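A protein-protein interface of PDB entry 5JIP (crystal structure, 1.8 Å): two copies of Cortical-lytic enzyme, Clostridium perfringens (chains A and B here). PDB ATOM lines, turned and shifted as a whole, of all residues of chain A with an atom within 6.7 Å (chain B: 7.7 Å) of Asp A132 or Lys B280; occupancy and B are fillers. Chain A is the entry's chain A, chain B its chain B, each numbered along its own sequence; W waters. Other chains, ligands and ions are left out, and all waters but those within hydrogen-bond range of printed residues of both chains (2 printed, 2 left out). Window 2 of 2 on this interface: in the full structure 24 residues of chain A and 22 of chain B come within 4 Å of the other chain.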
ATOM      1  N   ALA A  85     -23.804  26.046  10.235  1.00  0.00           N
ATOM      2  CA  ALA A  85     -22.608  26.829   9.930  1.00  0.00           C
ATOM      3  C   ALA A  85     -22.468  27.036   8.431  1.00  0.00           C
ATOM      4  O   ALA A  85     -22.092  28.130   7.979  1.00  0.00           O
ATOM      5  CB  ALA A  85     -21.367  26.157  10.504  1.00  0.00           C
ATOM      6  N   LEU A 112     -16.407  36.796  11.062  1.00  0.00           N
ATOM      7  CA  LEU A 112     -17.379  36.049  11.853  1.00  0.00           C
ATOM      8  C   LEU A 112     -17.329  36.532  13.300  1.00  0.00           C
ATOM      9  O   LEU A 112     -16.293  36.441  13.961  1.00  0.00           O
ATOM     10  CB  LEU A 112     -17.107  34.548  11.773  1.00  0.00           C
ATOM     11  CG  LEU A 112     -18.056  33.634  12.546  1.00  0.00           C
ATOM     12  CD1 LEU A 112     -19.408  33.617  11.878  1.00  0.00           C
ATOM     13  CD2 LEU A 112     -17.453  32.239  12.574  1.00  0.00           C
ATOM     14  N   LEU A 127     -18.490  24.209  19.905  1.00  0.00           N
ATOM     15  CA  LEU A 127     -18.434  25.603  19.461  1.00  0.00           C
ATOM     16  C   LEU A 127     -17.339  25.781  18.416  1.00  0.00           C
ATOM     17  O   LEU A 127     -17.571  26.347  17.344  1.00  0.00           O
ATOM     18  CB  LEU A 127     -18.200  26.532  20.641  1.00  0.00           C
ATOM     19  CG  LEU A 127     -18.073  28.025  20.310  1.00  0.00           C
ATOM     20  CD1 LEU A 127     -19.334  28.536  19.669  1.00  0.00           C
ATOM     21  CD2 LEU A 127     -17.784  28.869  21.546  1.00  0.00           C
ATOM     22  N   VAL A 128     -16.146  25.265  18.697  1.00  0.00           N
ATOM     23  CA  VAL A 128     -15.039  25.435  17.769  1.00  0.00           C
ATOM     24  C   VAL A 128     -15.319  24.700  16.460  1.00  0.00           C
ATOM     25  O   VAL A 128     -15.024  25.221  15.388  1.00  0.00           O
ATOM     26  CB  VAL A 128     -13.712  24.989  18.424  1.00  0.00           C
ATOM     27  CG1 VAL A 128     -12.584  24.935  17.408  1.00  0.00           C
ATOM     28  CG2 VAL A 128     -13.295  25.920  19.592  1.00  0.00           C
ATOM     29  N   ASN A 129     -15.851  23.466  16.515  1.00  0.00           N
ATOM     30  CA  ASN A 129     -16.228  22.777  15.289  1.00  0.00           C
ATOM     31  C   ASN A 129     -17.189  23.613  14.440  1.00  0.00           C
ATOM     32  O   ASN A 129     -17.102  23.612  13.206  1.00  0.00           O
ATOM     33  CB  ASN A 129     -16.863  21.428  15.610  1.00  0.00           C
ATOM     34  CG  ASN A 129     -15.841  20.372  15.949  1.00  0.00           C
ATOM     35  OD1 ASN A 129     -14.626  20.608  15.886  1.00  0.00           O
ATOM     36  ND2 ASN A 129     -16.326  19.194  16.298  1.00  0.00           N
ATOM     37  N   TRP A 130     -18.133  24.303  15.079  1.00  0.00           N
ATOM     38  CA  TRP A 130     -19.080  25.126  14.327  1.00  0.00           C
ATOM     39  C   TRP A 130     -18.375  26.291  13.639  1.00  0.00           C
ATOM     40  O   TRP A 130     -18.577  26.535  12.450  1.00  0.00           O
ATOM     41  CB  TRP A 130     -20.186  25.624  15.258  1.00  0.00           C
ATOM     42  CG  TRP A 130     -21.291  26.280  14.535  1.00  0.00           C
ATOM     43  CD1 TRP A 130     -22.479  25.714  14.140  1.00  0.00           C
ATOM     44  CD2 TRP A 130     -21.332  27.640  14.087  1.00  0.00           C
ATOM     45  NE1 TRP A 130     -23.240  26.639  13.473  1.00  0.00           N
ATOM     46  CE2 TRP A 130     -22.559  27.829  13.429  1.00  0.00           C
ATOM     47  CE3 TRP A 130     -20.439  28.721  14.178  1.00  0.00           C
ATOM     48  CZ2 TRP A 130     -22.934  29.073  12.880  1.00  0.00           C
ATOM     49  CZ3 TRP A 130     -20.806  29.932  13.628  1.00  0.00           C
ATOM     50  CH2 TRP A 130     -22.048  30.100  12.992  1.00  0.00           C
ATOM     51  N   ILE A 131     -17.511  27.000  14.370  1.00  0.00           N
ATOM     52  CA  ILE A 131     -16.740  28.088  13.778  1.00  0.00           C
ATOM     53  C   ILE A 131     -15.878  27.574  12.632  1.00  0.00           C
ATOM     54  O   ILE A 131     -15.824  28.164  11.550  1.00  0.00           O
ATOM     55  CB  ILE A 131     -15.882  28.758  14.856  1.00  0.00           C
ATOM     56  CG1 ILE A 131     -16.785  29.362  15.914  1.00  0.00           C
ATOM     57  CG2 ILE A 131     -14.907  29.770  14.218  1.00  0.00           C
ATOM     58  CD1 ILE A 131     -16.016  29.849  17.115  1.00  0.00           C
ATOM     59  N   ASP A 132     -15.180  26.466  12.870  1.00  0.00           N
ATOM     60  CA  ASP A 132     -14.272  25.890  11.889  1.00  0.00           C
ATOM     61  C   ASP A 132     -15.017  25.490  10.619  1.00  0.00           C
ATOM     62  O   ASP A 132     -14.499  25.634   9.510  1.00  0.00           O
ATOM     63  CB  ASP A 132     -13.589  24.686  12.547  1.00  0.00           C
ATOM     64  CG  ASP A 132     -12.264  24.317  11.907  1.00  0.00           C
ATOM     65  OD1 ASP A 132     -11.639  25.157  11.228  1.00  0.00           O
ATOM     66  OD2 ASP A 132     -11.850  23.160  12.111  1.00  0.00           O
ATOM     67  N   ARG A 133     -16.243  24.972  10.761  1.00  0.00           N
ATOM     68  CA  ARG A 133     -17.022  24.614   9.589  1.00  0.00           C
ATOM     69  C   ARG A 133     -17.436  25.855   8.818  1.00  0.00           C
ATOM     70  O   ARG A 133     -17.404  25.869   7.580  1.00  0.00           O
ATOM     71  CB  ARG A 133     -18.262  23.812  10.014  1.00  0.00           C
ATOM     72  CG  ARG A 133     -19.269  23.569   8.885  1.00  0.00           C
ATOM     73  CD  ARG A 133     -18.703  22.689   7.768  1.00  0.00           C
ATOM     74  NE  ARG A 133     -18.269  21.394   8.290  1.00  0.00           N
ATOM     75  CZ  ARG A 133     -19.039  20.308   8.361  1.00  0.00           C
ATOM     76  NH1 ARG A 133     -18.544  19.177   8.857  1.00  0.00           N
ATOM     77  NH2 ARG A 133     -20.300  20.340   7.937  1.00  0.00           N
ATOM     78  N   PHE A 134     -17.856  26.889   9.542  1.00  0.00           N
ATOM     79  CA  PHE A 134     -18.181  28.169   8.914  1.00  0.00           C
ATOM     80  C   PHE A 134     -16.972  28.693   8.148  1.00  0.00           C
ATOM     81  O   PHE A 134     -17.066  29.033   6.964  1.00  0.00           O
ATOM     82  CB  PHE A 134     -18.631  29.161   9.983  1.00  0.00           C
ATOM     83  CG  PHE A 134     -19.162  30.477   9.424  1.00  0.00           C
ATOM     84  CD1 PHE A 134     -18.307  31.424   8.872  1.00  0.00           C
ATOM     85  CD2 PHE A 134     -20.514  30.758   9.467  1.00  0.00           C
ATOM     86  CE1 PHE A 134     -18.801  32.637   8.355  1.00  0.00           C
ATOM     87  CE2 PHE A 134     -21.017  31.984   8.963  1.00  0.00           C
ATOM     88  CZ  PHE A 134     -20.155  32.910   8.407  1.00  0.00           C
ATOM     89  N   ARG A 135     -15.808  28.680   8.790  1.00  0.00           N
ATOM     90  CA  ARG A 135     -14.576  29.100   8.122  1.00  0.00           C
ATOM     91  C   ARG A 135     -14.299  28.284   6.855  1.00  0.00           C
ATOM     92  O   ARG A 135     -13.946  28.843   5.802  1.00  0.00           O
ATOM     93  CB  ARG A 135     -13.417  28.999   9.112  1.00  0.00           C
ATOM     94  CG  ARG A 135     -12.048  29.339   8.543  1.00  0.00           C
ATOM     95  CD  ARG A 135     -11.260  28.105   8.218  1.00  0.00           C
ATOM     96  NE  ARG A 135     -10.877  27.402   9.448  1.00  0.00           N
ATOM     97  CZ  ARG A 135      -9.742  27.575  10.122  1.00  0.00           C
ATOM     98  NH1 ARG A 135      -8.819  28.405   9.679  1.00  0.00           N
ATOM     99  NH2 ARG A 135      -9.517  26.883  11.240  1.00  0.00           N
ATOM    100  N   ASP A 136     -14.426  26.954   6.931  1.00  0.00           N
ATOM    101  CA  ASP A 136     -14.138  26.125   5.759  1.00  0.00           C
ATOM    102  C   ASP A 136     -15.066  26.459   4.597  1.00  0.00           C
ATOM    103  O   ASP A 136     -14.630  26.580   3.444  1.00  0.00           O
ATOM    104  CB  ASP A 136     -14.251  24.629   6.113  1.00  0.00           C
ATOM    105  CG  ASP A 136     -13.099  24.127   6.965  1.00  0.00           C
ATOM    106  OD1 ASP A 136     -12.066  24.822   7.077  1.00  0.00           O
ATOM    107  OD2 ASP A 136     -13.226  23.018   7.523  1.00  0.00           O
ATOM    108  N   ARG A 137     -16.360  26.567   4.866  1.00  0.00           N
ATOM    109  CA  ARG A 137     -17.302  26.925   3.815  1.00  0.00           C
ATOM    110  C   ARG A 137     -17.001  28.304   3.261  1.00  0.00           C
ATOM    111  O   ARG A 137     -16.962  28.505   2.039  1.00  0.00           O
ATOM    112  CB  ARG A 137     -18.729  26.877   4.355  1.00  0.00           C
ATOM    113  CG  ARG A 137     -19.813  27.186   3.328  1.00  0.00           C
ATOM    114  CD  ARG A 137     -19.836  26.134   2.249  1.00  0.00           C
ATOM    115  NE  ARG A 137     -21.080  26.200   1.497  1.00  0.00           N
ATOM    116  CZ  ARG A 137     -21.560  25.206   0.761  1.00  0.00           C
ATOM    117  NH1 ARG A 137     -20.885  24.057   0.661  1.00  0.00           N
ATOM    118  NH2 ARG A 137     -22.711  25.376   0.120  1.00  0.00           N
ATOM    119  N   PRO A 169      -7.624  24.713  17.060  1.00  0.00           N
ATOM    120  CA  PRO A 169      -7.885  24.658  15.615  1.00  0.00           C
ATOM    121  C   PRO A 169      -8.139  26.012  14.969  1.00  0.00           C
ATOM    122  O   PRO A 169      -8.010  26.121  13.744  1.00  0.00           O
ATOM    123  CB  PRO A 169      -9.128  23.763  15.514  1.00  0.00           C
ATOM    124  CG  PRO A 169      -9.152  22.970  16.831  1.00  0.00           C
ATOM    125  CD  PRO A 169      -8.599  23.925  17.835  1.00  0.00           C
ATOM    126  N   LEU A 170      -8.537  27.030  15.724  1.00  0.00           N
ATOM    127  CA  LEU A 170      -8.823  28.327  15.107  1.00  0.00           C
ATOM    128  C   LEU A 170      -7.636  29.288  15.131  1.00  0.00           C
ATOM    129  O   LEU A 170      -7.783  30.435  14.675  1.00  0.00           O
ATOM    130  CB  LEU A 170     -10.009  28.975  15.802  1.00  0.00           C
ATOM    131  CG  LEU A 170     -11.243  28.097  15.932  1.00  0.00           C
ATOM    132  CD1 LEU A 170     -12.297  28.825  16.733  1.00  0.00           C
ATOM    133  CD2 LEU A 170     -11.761  27.602  14.577  1.00  0.00           C
ATOM    134  N   ASP A 172      -5.079  29.707  13.466  1.00  0.00           N
ATOM    135  CA  ASP A 172      -4.586  30.205  12.200  1.00  0.00           C
ATOM    136  C   ASP A 172      -5.536  31.243  11.609  1.00  0.00           C
ATOM    137  O   ASP A 172      -5.185  31.889  10.630  1.00  0.00           O
ATOM    138  CB  ASP A 172      -4.355  29.057  11.200  1.00  0.00           C
ATOM    139  CG  ASP A 172      -5.635  28.390  10.740  1.00  0.00           C
ATOM    140  OD1 ASP A 172      -6.546  28.171  11.577  1.00  0.00           O
ATOM    141  OD2 ASP A 172      -5.700  28.071   9.528  1.00  0.00           O
ATOM    142  N   MET A 173      -6.694  31.468  12.219  1.00  0.00           N
ATOM    143  CA  MET A 173      -7.548  32.561  11.769  1.00  0.00           C
ATOM    144  C   MET A 173      -6.967  33.905  12.200  1.00  0.00           C
ATOM    145  O   MET A 173      -6.413  34.022  13.286  1.00  0.00           O
ATOM    146  CB  MET A 173      -8.965  32.411  12.338  1.00  0.00           C
ATOM    147  CG  MET A 173      -9.628  31.123  11.935  1.00  0.00           C
ATOM    148  SD  MET A 173     -11.336  31.077  12.504  1.00  0.00           S
ATOM    149  CE  MET A 173     -12.103  32.300  11.407  1.00  0.00           C
ATOM    150  N   ASN B 239      -2.915  14.079   3.875  1.00  0.00           N
ATOM    151  CA  ASN B 239      -4.086  13.216   3.860  1.00  0.00           C
ATOM    152  C   ASN B 239      -5.178  13.853   3.017  1.00  0.00           C
ATOM    153  O   ASN B 239      -5.331  15.073   3.006  1.00  0.00           O
ATOM    154  CB  ASN B 239      -4.590  12.999   5.285  1.00  0.00           C
ATOM    155  CG  ASN B 239      -5.821  12.167   5.327  1.00  0.00           C
ATOM    156  OD1 ASN B 239      -5.810  11.026   4.899  1.00  0.00           O
ATOM    157  ND2 ASN B 239      -6.880  12.717   5.865  1.00  0.00           N
ATOM    158  N   PHE B 248     -11.203  17.002   0.611  1.00  0.00           N
ATOM    159  CA  PHE B 248     -10.731  17.611   1.845  1.00  0.00           C
ATOM    160  C   PHE B 248      -9.287  17.172   2.041  1.00  0.00           C
ATOM    161  O   PHE B 248      -9.013  15.977   2.180  1.00  0.00           O
ATOM    162  CB  PHE B 248     -11.602  17.195   3.028  1.00  0.00           C
ATOM    163  CG  PHE B 248     -13.005  17.710   2.944  1.00  0.00           C
ATOM    164  CD1 PHE B 248     -13.937  17.090   2.131  1.00  0.00           C
ATOM    165  CD2 PHE B 248     -13.389  18.807   3.690  1.00  0.00           C
ATOM    166  CE1 PHE B 248     -15.248  17.561   2.062  1.00  0.00           C
ATOM    167  CE2 PHE B 248     -14.692  19.278   3.634  1.00  0.00           C
ATOM    168  CZ  PHE B 248     -15.623  18.646   2.815  1.00  0.00           C
ATOM    169  N   VAL B 249      -8.370  18.128   1.996  1.00  0.00           N
ATOM    170  CA  VAL B 249      -6.940  17.860   2.090  1.00  0.00           C
ATOM    171  C   VAL B 249      -6.424  18.470   3.384  1.00  0.00           C
ATOM    172  O   VAL B 249      -6.802  19.590   3.739  1.00  0.00           O
ATOM    173  CB  VAL B 249      -6.180  18.438   0.878  1.00  0.00           C
ATOM    174  CG1 VAL B 249      -4.716  18.063   0.933  1.00  0.00           C
ATOM    175  CG2 VAL B 249      -6.840  17.970  -0.444  1.00  0.00           C
ATOM    176  N   ASN B 250      -5.574  17.731   4.093  1.00  0.00           N
ATOM    177  CA  ASN B 250      -4.894  18.292   5.255  1.00  0.00           C
ATOM    178  C   ASN B 250      -3.463  17.775   5.304  1.00  0.00           C
ATOM    179  O   ASN B 250      -3.101  16.775   4.666  1.00  0.00           O
ATOM    180  CB  ASN B 250      -5.639  17.995   6.575  1.00  0.00           C
ATOM    181  CG  ASN B 250      -5.586  16.525   6.977  1.00  0.00           C
ATOM    182  OD1 ASN B 250      -6.176  15.675   6.330  1.00  0.00           O
ATOM    183  ND2 ASN B 250      -4.897  16.238   8.069  1.00  0.00           N
ATOM    184  N   TRP B 251      -2.642  18.469   6.093  1.00  0.00           N
ATOM    185  CA  TRP B 251      -1.243  18.090   6.215  1.00  0.00           C
ATOM    186  C   TRP B 251      -0.733  18.603   7.545  1.00  0.00           C
ATOM    187  O   TRP B 251      -1.383  19.403   8.222  1.00  0.00           O
ATOM    188  CB  TRP B 251      -0.412  18.619   5.034  1.00  0.00           C
ATOM    189  CG  TRP B 251      -0.559  20.125   4.824  1.00  0.00           C
ATOM    190  CD1 TRP B 251       0.210  21.120   5.378  1.00  0.00           C
ATOM    191  CD2 TRP B 251      -1.535  20.777   4.006  1.00  0.00           C
ATOM    192  NE1 TRP B 251      -0.262  22.366   4.975  1.00  0.00           N
ATOM    193  CE2 TRP B 251      -1.332  22.171   4.135  1.00  0.00           C
ATOM    194  CE3 TRP B 251      -2.603  20.323   3.213  1.00  0.00           C
ATOM    195  CZ2 TRP B 251      -2.127  23.102   3.468  1.00  0.00           C
ATOM    196  CZ3 TRP B 251      -3.381  21.272   2.557  1.00  0.00           C
ATOM    197  CH2 TRP B 251      -3.130  22.625   2.684  1.00  0.00           C
ATOM    198  N   THR B 252       0.437  18.113   7.916  1.00  0.00           N
ATOM    199  CA  THR B 252       1.125  18.634   9.080  1.00  0.00           C
ATOM    200  C   THR B 252       1.786  19.959   8.725  1.00  0.00           C
ATOM    201  O   THR B 252       2.302  20.127   7.617  1.00  0.00           O
ATOM    202  CB  THR B 252       2.155  17.613   9.553  1.00  0.00           C
ATOM    203  OG1 THR B 252       1.458  16.399   9.865  1.00  0.00           O
ATOM    204  CG2 THR B 252       2.948  18.130  10.769  1.00  0.00           C
ATOM    205  N   TYR B 262       2.155  27.253   1.021  1.00  0.00           N
ATOM    206  CA  TYR B 262       2.068  25.992   0.305  1.00  0.00           C
ATOM    207  C   TYR B 262       1.329  26.232  -0.998  1.00  0.00           C
ATOM    208  O   TYR B 262       0.435  27.073  -1.069  1.00  0.00           O
ATOM    209  CB  TYR B 262       1.300  24.921   1.101  1.00  0.00           C
ATOM    210  CG  TYR B 262       1.753  24.728   2.527  1.00  0.00           C
ATOM    211  CD1 TYR B 262       1.294  25.551   3.554  1.00  0.00           C
ATOM    212  CD2 TYR B 262       2.622  23.695   2.857  1.00  0.00           C
ATOM    213  CE1 TYR B 262       1.723  25.387   4.857  1.00  0.00           C
ATOM    214  CE2 TYR B 262       3.052  23.505   4.173  1.00  0.00           C
ATOM    215  CZ  TYR B 262       2.582  24.339   5.173  1.00  0.00           C
ATOM    216  OH  TYR B 262       3.000  24.129   6.488  1.00  0.00           O
ATOM    217  N   VAL B 264      -0.913  23.701  -3.585  1.00  0.00           N
ATOM    218  CA  VAL B 264      -1.560  22.396  -3.663  1.00  0.00           C
ATOM    219  C   VAL B 264      -1.976  22.176  -5.105  1.00  0.00           C
ATOM    220  O   VAL B 264      -2.374  23.125  -5.784  1.00  0.00           O
ATOM    221  CB  VAL B 264      -2.778  22.284  -2.726  1.00  0.00           C
ATOM    222  CG1 VAL B 264      -3.522  20.949  -2.935  1.00  0.00           C
ATOM    223  CG2 VAL B 264      -2.323  22.414  -1.276  1.00  0.00           C
ATOM    224  N   LEU B 274      -1.764  28.563  -0.044  1.00  0.00           N
ATOM    225  CA  LEU B 274      -2.143  28.673   1.356  1.00  0.00           C
ATOM    226  C   LEU B 274      -1.040  29.403   2.099  1.00  0.00           C
ATOM    227  O   LEU B 274       0.124  29.315   1.701  1.00  0.00           O
ATOM    228  CB  LEU B 274      -2.363  27.309   2.030  1.00  0.00           C
ATOM    229  CG  LEU B 274      -3.517  26.400   1.577  1.00  0.00           C
ATOM    230  CD1 LEU B 274      -4.844  27.155   1.469  1.00  0.00           C
ATOM    231  CD2 LEU B 274      -3.149  25.706   0.247  1.00  0.00           C
ATOM    232  N   PRO B 275      -1.378  30.164   3.137  1.00  0.00           N
ATOM    233  CA  PRO B 275      -0.373  30.887   3.923  1.00  0.00           C
ATOM    234  C   PRO B 275       0.316  29.956   4.922  1.00  0.00           C
ATOM    235  O   PRO B 275       0.014  28.773   5.010  1.00  0.00           O
ATOM    236  CB  PRO B 275      -1.201  31.973   4.627  1.00  0.00           C
ATOM    237  CG  PRO B 275      -2.516  31.280   4.841  1.00  0.00           C
ATOM    238  CD  PRO B 275      -2.746  30.478   3.592  1.00  0.00           C
ATOM    239  N   LYS B 277       0.508  29.373   8.130  1.00  0.00           N
ATOM    240  CA  LYS B 277      -0.130  28.659   9.237  1.00  0.00           C
ATOM    241  C   LYS B 277      -1.162  27.632   8.787  1.00  0.00           C
ATOM    242  O   LYS B 277      -1.703  26.903   9.628  1.00  0.00           O
ATOM    243  CB  LYS B 277      -0.769  29.655  10.212  1.00  0.00           C
ATOM    244  CG  LYS B 277       0.215  30.549  10.968  1.00  0.00           C
ATOM    245  CD  LYS B 277      -0.520  31.551  11.854  1.00  0.00           C
ATOM    246  CE  LYS B 277       0.425  32.360  12.759  1.00  0.00           C
ATOM    247  NZ  LYS B 277       1.579  32.976  12.047  1.00  0.00           N
ATOM    248  N   ALA B 278      -1.385  27.491   7.485  1.00  0.00           N
ATOM    249  CA  ALA B 278      -2.447  26.646   6.969  1.00  0.00           C
ATOM    250  C   ALA B 278      -2.079  25.166   7.058  1.00  0.00           C
ATOM    251  O   ALA B 278      -0.923  24.786   6.867  1.00  0.00           O
ATOM    252  CB  ALA B 278      -2.753  26.997   5.513  1.00  0.00           C
ATOM    253  N   THR B 279      -3.100  24.331   7.302  1.00  0.00           N
ATOM    254  CA  THR B 279      -2.907  22.886   7.323  1.00  0.00           C
ATOM    255  C   THR B 279      -4.008  22.141   6.585  1.00  0.00           C
ATOM    256  O   THR B 279      -4.084  20.897   6.696  1.00  0.00           O
ATOM    257  CB  THR B 279      -2.827  22.347   8.750  1.00  0.00           C
ATOM    258  OG1 THR B 279      -4.043  22.634   9.457  1.00  0.00           O
ATOM    259  CG2 THR B 279      -1.655  22.952   9.464  1.00  0.00           C
ATOM    260  N   LYS B 280      -4.847  22.841   5.827  1.00  0.00           N
ATOM    261  CA  LYS B 280      -5.906  22.196   5.075  1.00  0.00           C
ATOM    262  C   LYS B 280      -6.353  23.086   3.926  1.00  0.00           C
ATOM    263  O   LYS B 280      -6.135  24.296   3.934  1.00  0.00           O
ATOM    264  CB  LYS B 280      -7.096  21.891   5.967  1.00  0.00           C
ATOM    265  CG  LYS B 280      -7.647  23.082   6.689  1.00  0.00           C
ATOM    266  CD  LYS B 280      -8.765  22.627   7.631  1.00  0.00           C
ATOM    267  CE  LYS B 280      -9.260  23.778   8.496  1.00  0.00           C
ATOM    268  NZ  LYS B 280     -10.536  23.438   9.142  1.00  0.00           N
ATOM    269  N   ILE B 281      -7.000  22.454   2.947  1.00  0.00           N
ATOM    270  CA  ILE B 281      -7.725  23.158   1.895  1.00  0.00           C
ATOM    271  C   ILE B 281      -8.875  22.253   1.479  1.00  0.00           C
ATOM    272  O   ILE B 281      -8.754  21.028   1.488  1.00  0.00           O
ATOM    273  CB  ILE B 281      -6.810  23.520   0.704  1.00  0.00           C
ATOM    274  CG1 ILE B 281      -7.585  24.431  -0.271  1.00  0.00           C
ATOM    275  CG2 ILE B 281      -6.318  22.263   0.015  1.00  0.00           C
ATOM    276  CD1 ILE B 281      -6.794  24.915  -1.468  1.00  0.00           C
ATOM    277  N   VAL B 282     -10.007  22.863   1.154  1.00  0.00           N
ATOM    278  CA  VAL B 282     -11.181  22.160   0.652  1.00  0.00           C
ATOM    279  C   VAL B 282     -11.301  22.516  -0.823  1.00  0.00           C
ATOM    280  O   VAL B 282     -11.376  23.702  -1.173  1.00  0.00           O
ATOM    281  CB  VAL B 282     -12.460  22.533   1.423  1.00  0.00           C
ATOM    282  CG1 VAL B 282     -13.633  21.768   0.864  1.00  0.00           C
ATOM    283  CG2 VAL B 282     -12.306  22.240   2.930  1.00  0.00           C
ATOM    284  N   ILE B 283     -11.305  21.496  -1.685  1.00  0.00           N
ATOM    285  CA  ILE B 283     -11.268  21.671  -3.134  1.00  0.00           C
ATOM    286  C   ILE B 283     -12.577  21.179  -3.738  1.00  0.00           C
ATOM    287  O   ILE B 283     -12.955  20.023  -3.549  1.00  0.00           O
ATOM    288  CB  ILE B 283     -10.090  20.911  -3.755  1.00  0.00           C
ATOM    289  CG1 ILE B 283      -8.776  21.421  -3.159  1.00  0.00           C
ATOM    290  CG2 ILE B 283     -10.074  21.085  -5.282  1.00  0.00           C
ATOM    291  CD1 ILE B 283      -7.606  20.547  -3.516  1.00  0.00           C
ATOM    292  N   ILE B 300       1.552  18.527  -2.985  1.00  0.00           N
ATOM    293  CA  ILE B 300       1.741  19.756  -2.234  1.00  0.00           C
ATOM    294  C   ILE B 300       3.227  20.054  -2.131  1.00  0.00           C
ATOM    295  O   ILE B 300       4.067  19.153  -2.119  1.00  0.00           O
ATOM    296  CB  ILE B 300       1.073  19.662  -0.841  1.00  0.00           C
ATOM    297  CG1 ILE B 300       1.083  21.025  -0.158  1.00  0.00           C
ATOM    298  CG2 ILE B 300       1.758  18.571   0.022  1.00  0.00           C
ATOM    299  CD1 ILE B 300       0.307  21.044   1.140  1.00  0.00           C
HETATM  300  O   HOH W   1      -4.112  29.459   7.661  1.00  0.00           O
HETATM  301  O   HOH W   2      -5.574  25.821   7.895  1.00  0.00           O
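O of Pro A169 lies within hydrogen-bond range of NH2 of Arg A135 (3.0 Å).
The side-chain carboxylate of Asp A172 lies within salt-bridge range of the guanidinium group of Arg A135, 3.0 Å away.
The side-chain carboxylate of Asp A132 is in salt-bridge range of the guanidinium group of Arg A135 (2.7 Å).
The guanidinium group (NE) of Arg A135 is in salt-bridge range of the side-chain carboxylate (OD1) of Asp A136.
NE of Arg A135 touches NZ of Lys B280 (3.99 Å).
Asp A172 touches Lys B277 (CB to O, 3.8 Å).
No position is printed for both chains.
The side-chain carboxylate of Asp A132 is in salt-bridge range of the side-chain amino group of Lys B280 (2.9 Å).
The side-chain amino group (NZ) of Lys B280 lies within salt-bridge range of the side-chain carboxylate (OD1) of Asp A136 (2.9 Å).
Asp A132 touches just one residue of chain B: Lys B280.
Printed residues of chain B within 4 Å of Arg A135: Lys B280 (3.99 Å).
Printed residues of chain B within 4 Å of Asp A136: Lys B280 (2.9 Å).
Of the printed residues of chain B, Asp A172 touches Lys B277.
Of the printed residues of chain A, Lys B277 touches Asp A172 (3.8 Å).
Printed residues of chain A within 4 Å of Lys B280: Asp A132, Arg A135 and Asp A136.
The nearest printed residue of chain B that does not touch Asp A136 is Val B282 (4.4 Å).
Of the 18 printed residues of chain B, 2 touch a printed residue of chain A.
Printed residues of chain B that touch a printed residue of chain A: Lys B277 and Lys B280.
Of the 17 printed residues of chain A, 4 touch a printed residue of chain B.
Among the printed residues, Asp or Glu carboxylates within 4 Å of a Lys or Arg side-chain nitrogen of the other chain: Asp A132 with Lys B280 (2.9 Å) and Asp A136 with Lys B280 (2.9 Å).
Water W2 lies within hydrogen-bond range of OD2 of Asp A172 (2.8 Å) and N of Thr B279 (2.9 Å).
Water W1 bridges OD2 of Asp A172 (2.8 Å) and N of Ala B278 (3.4 Å).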
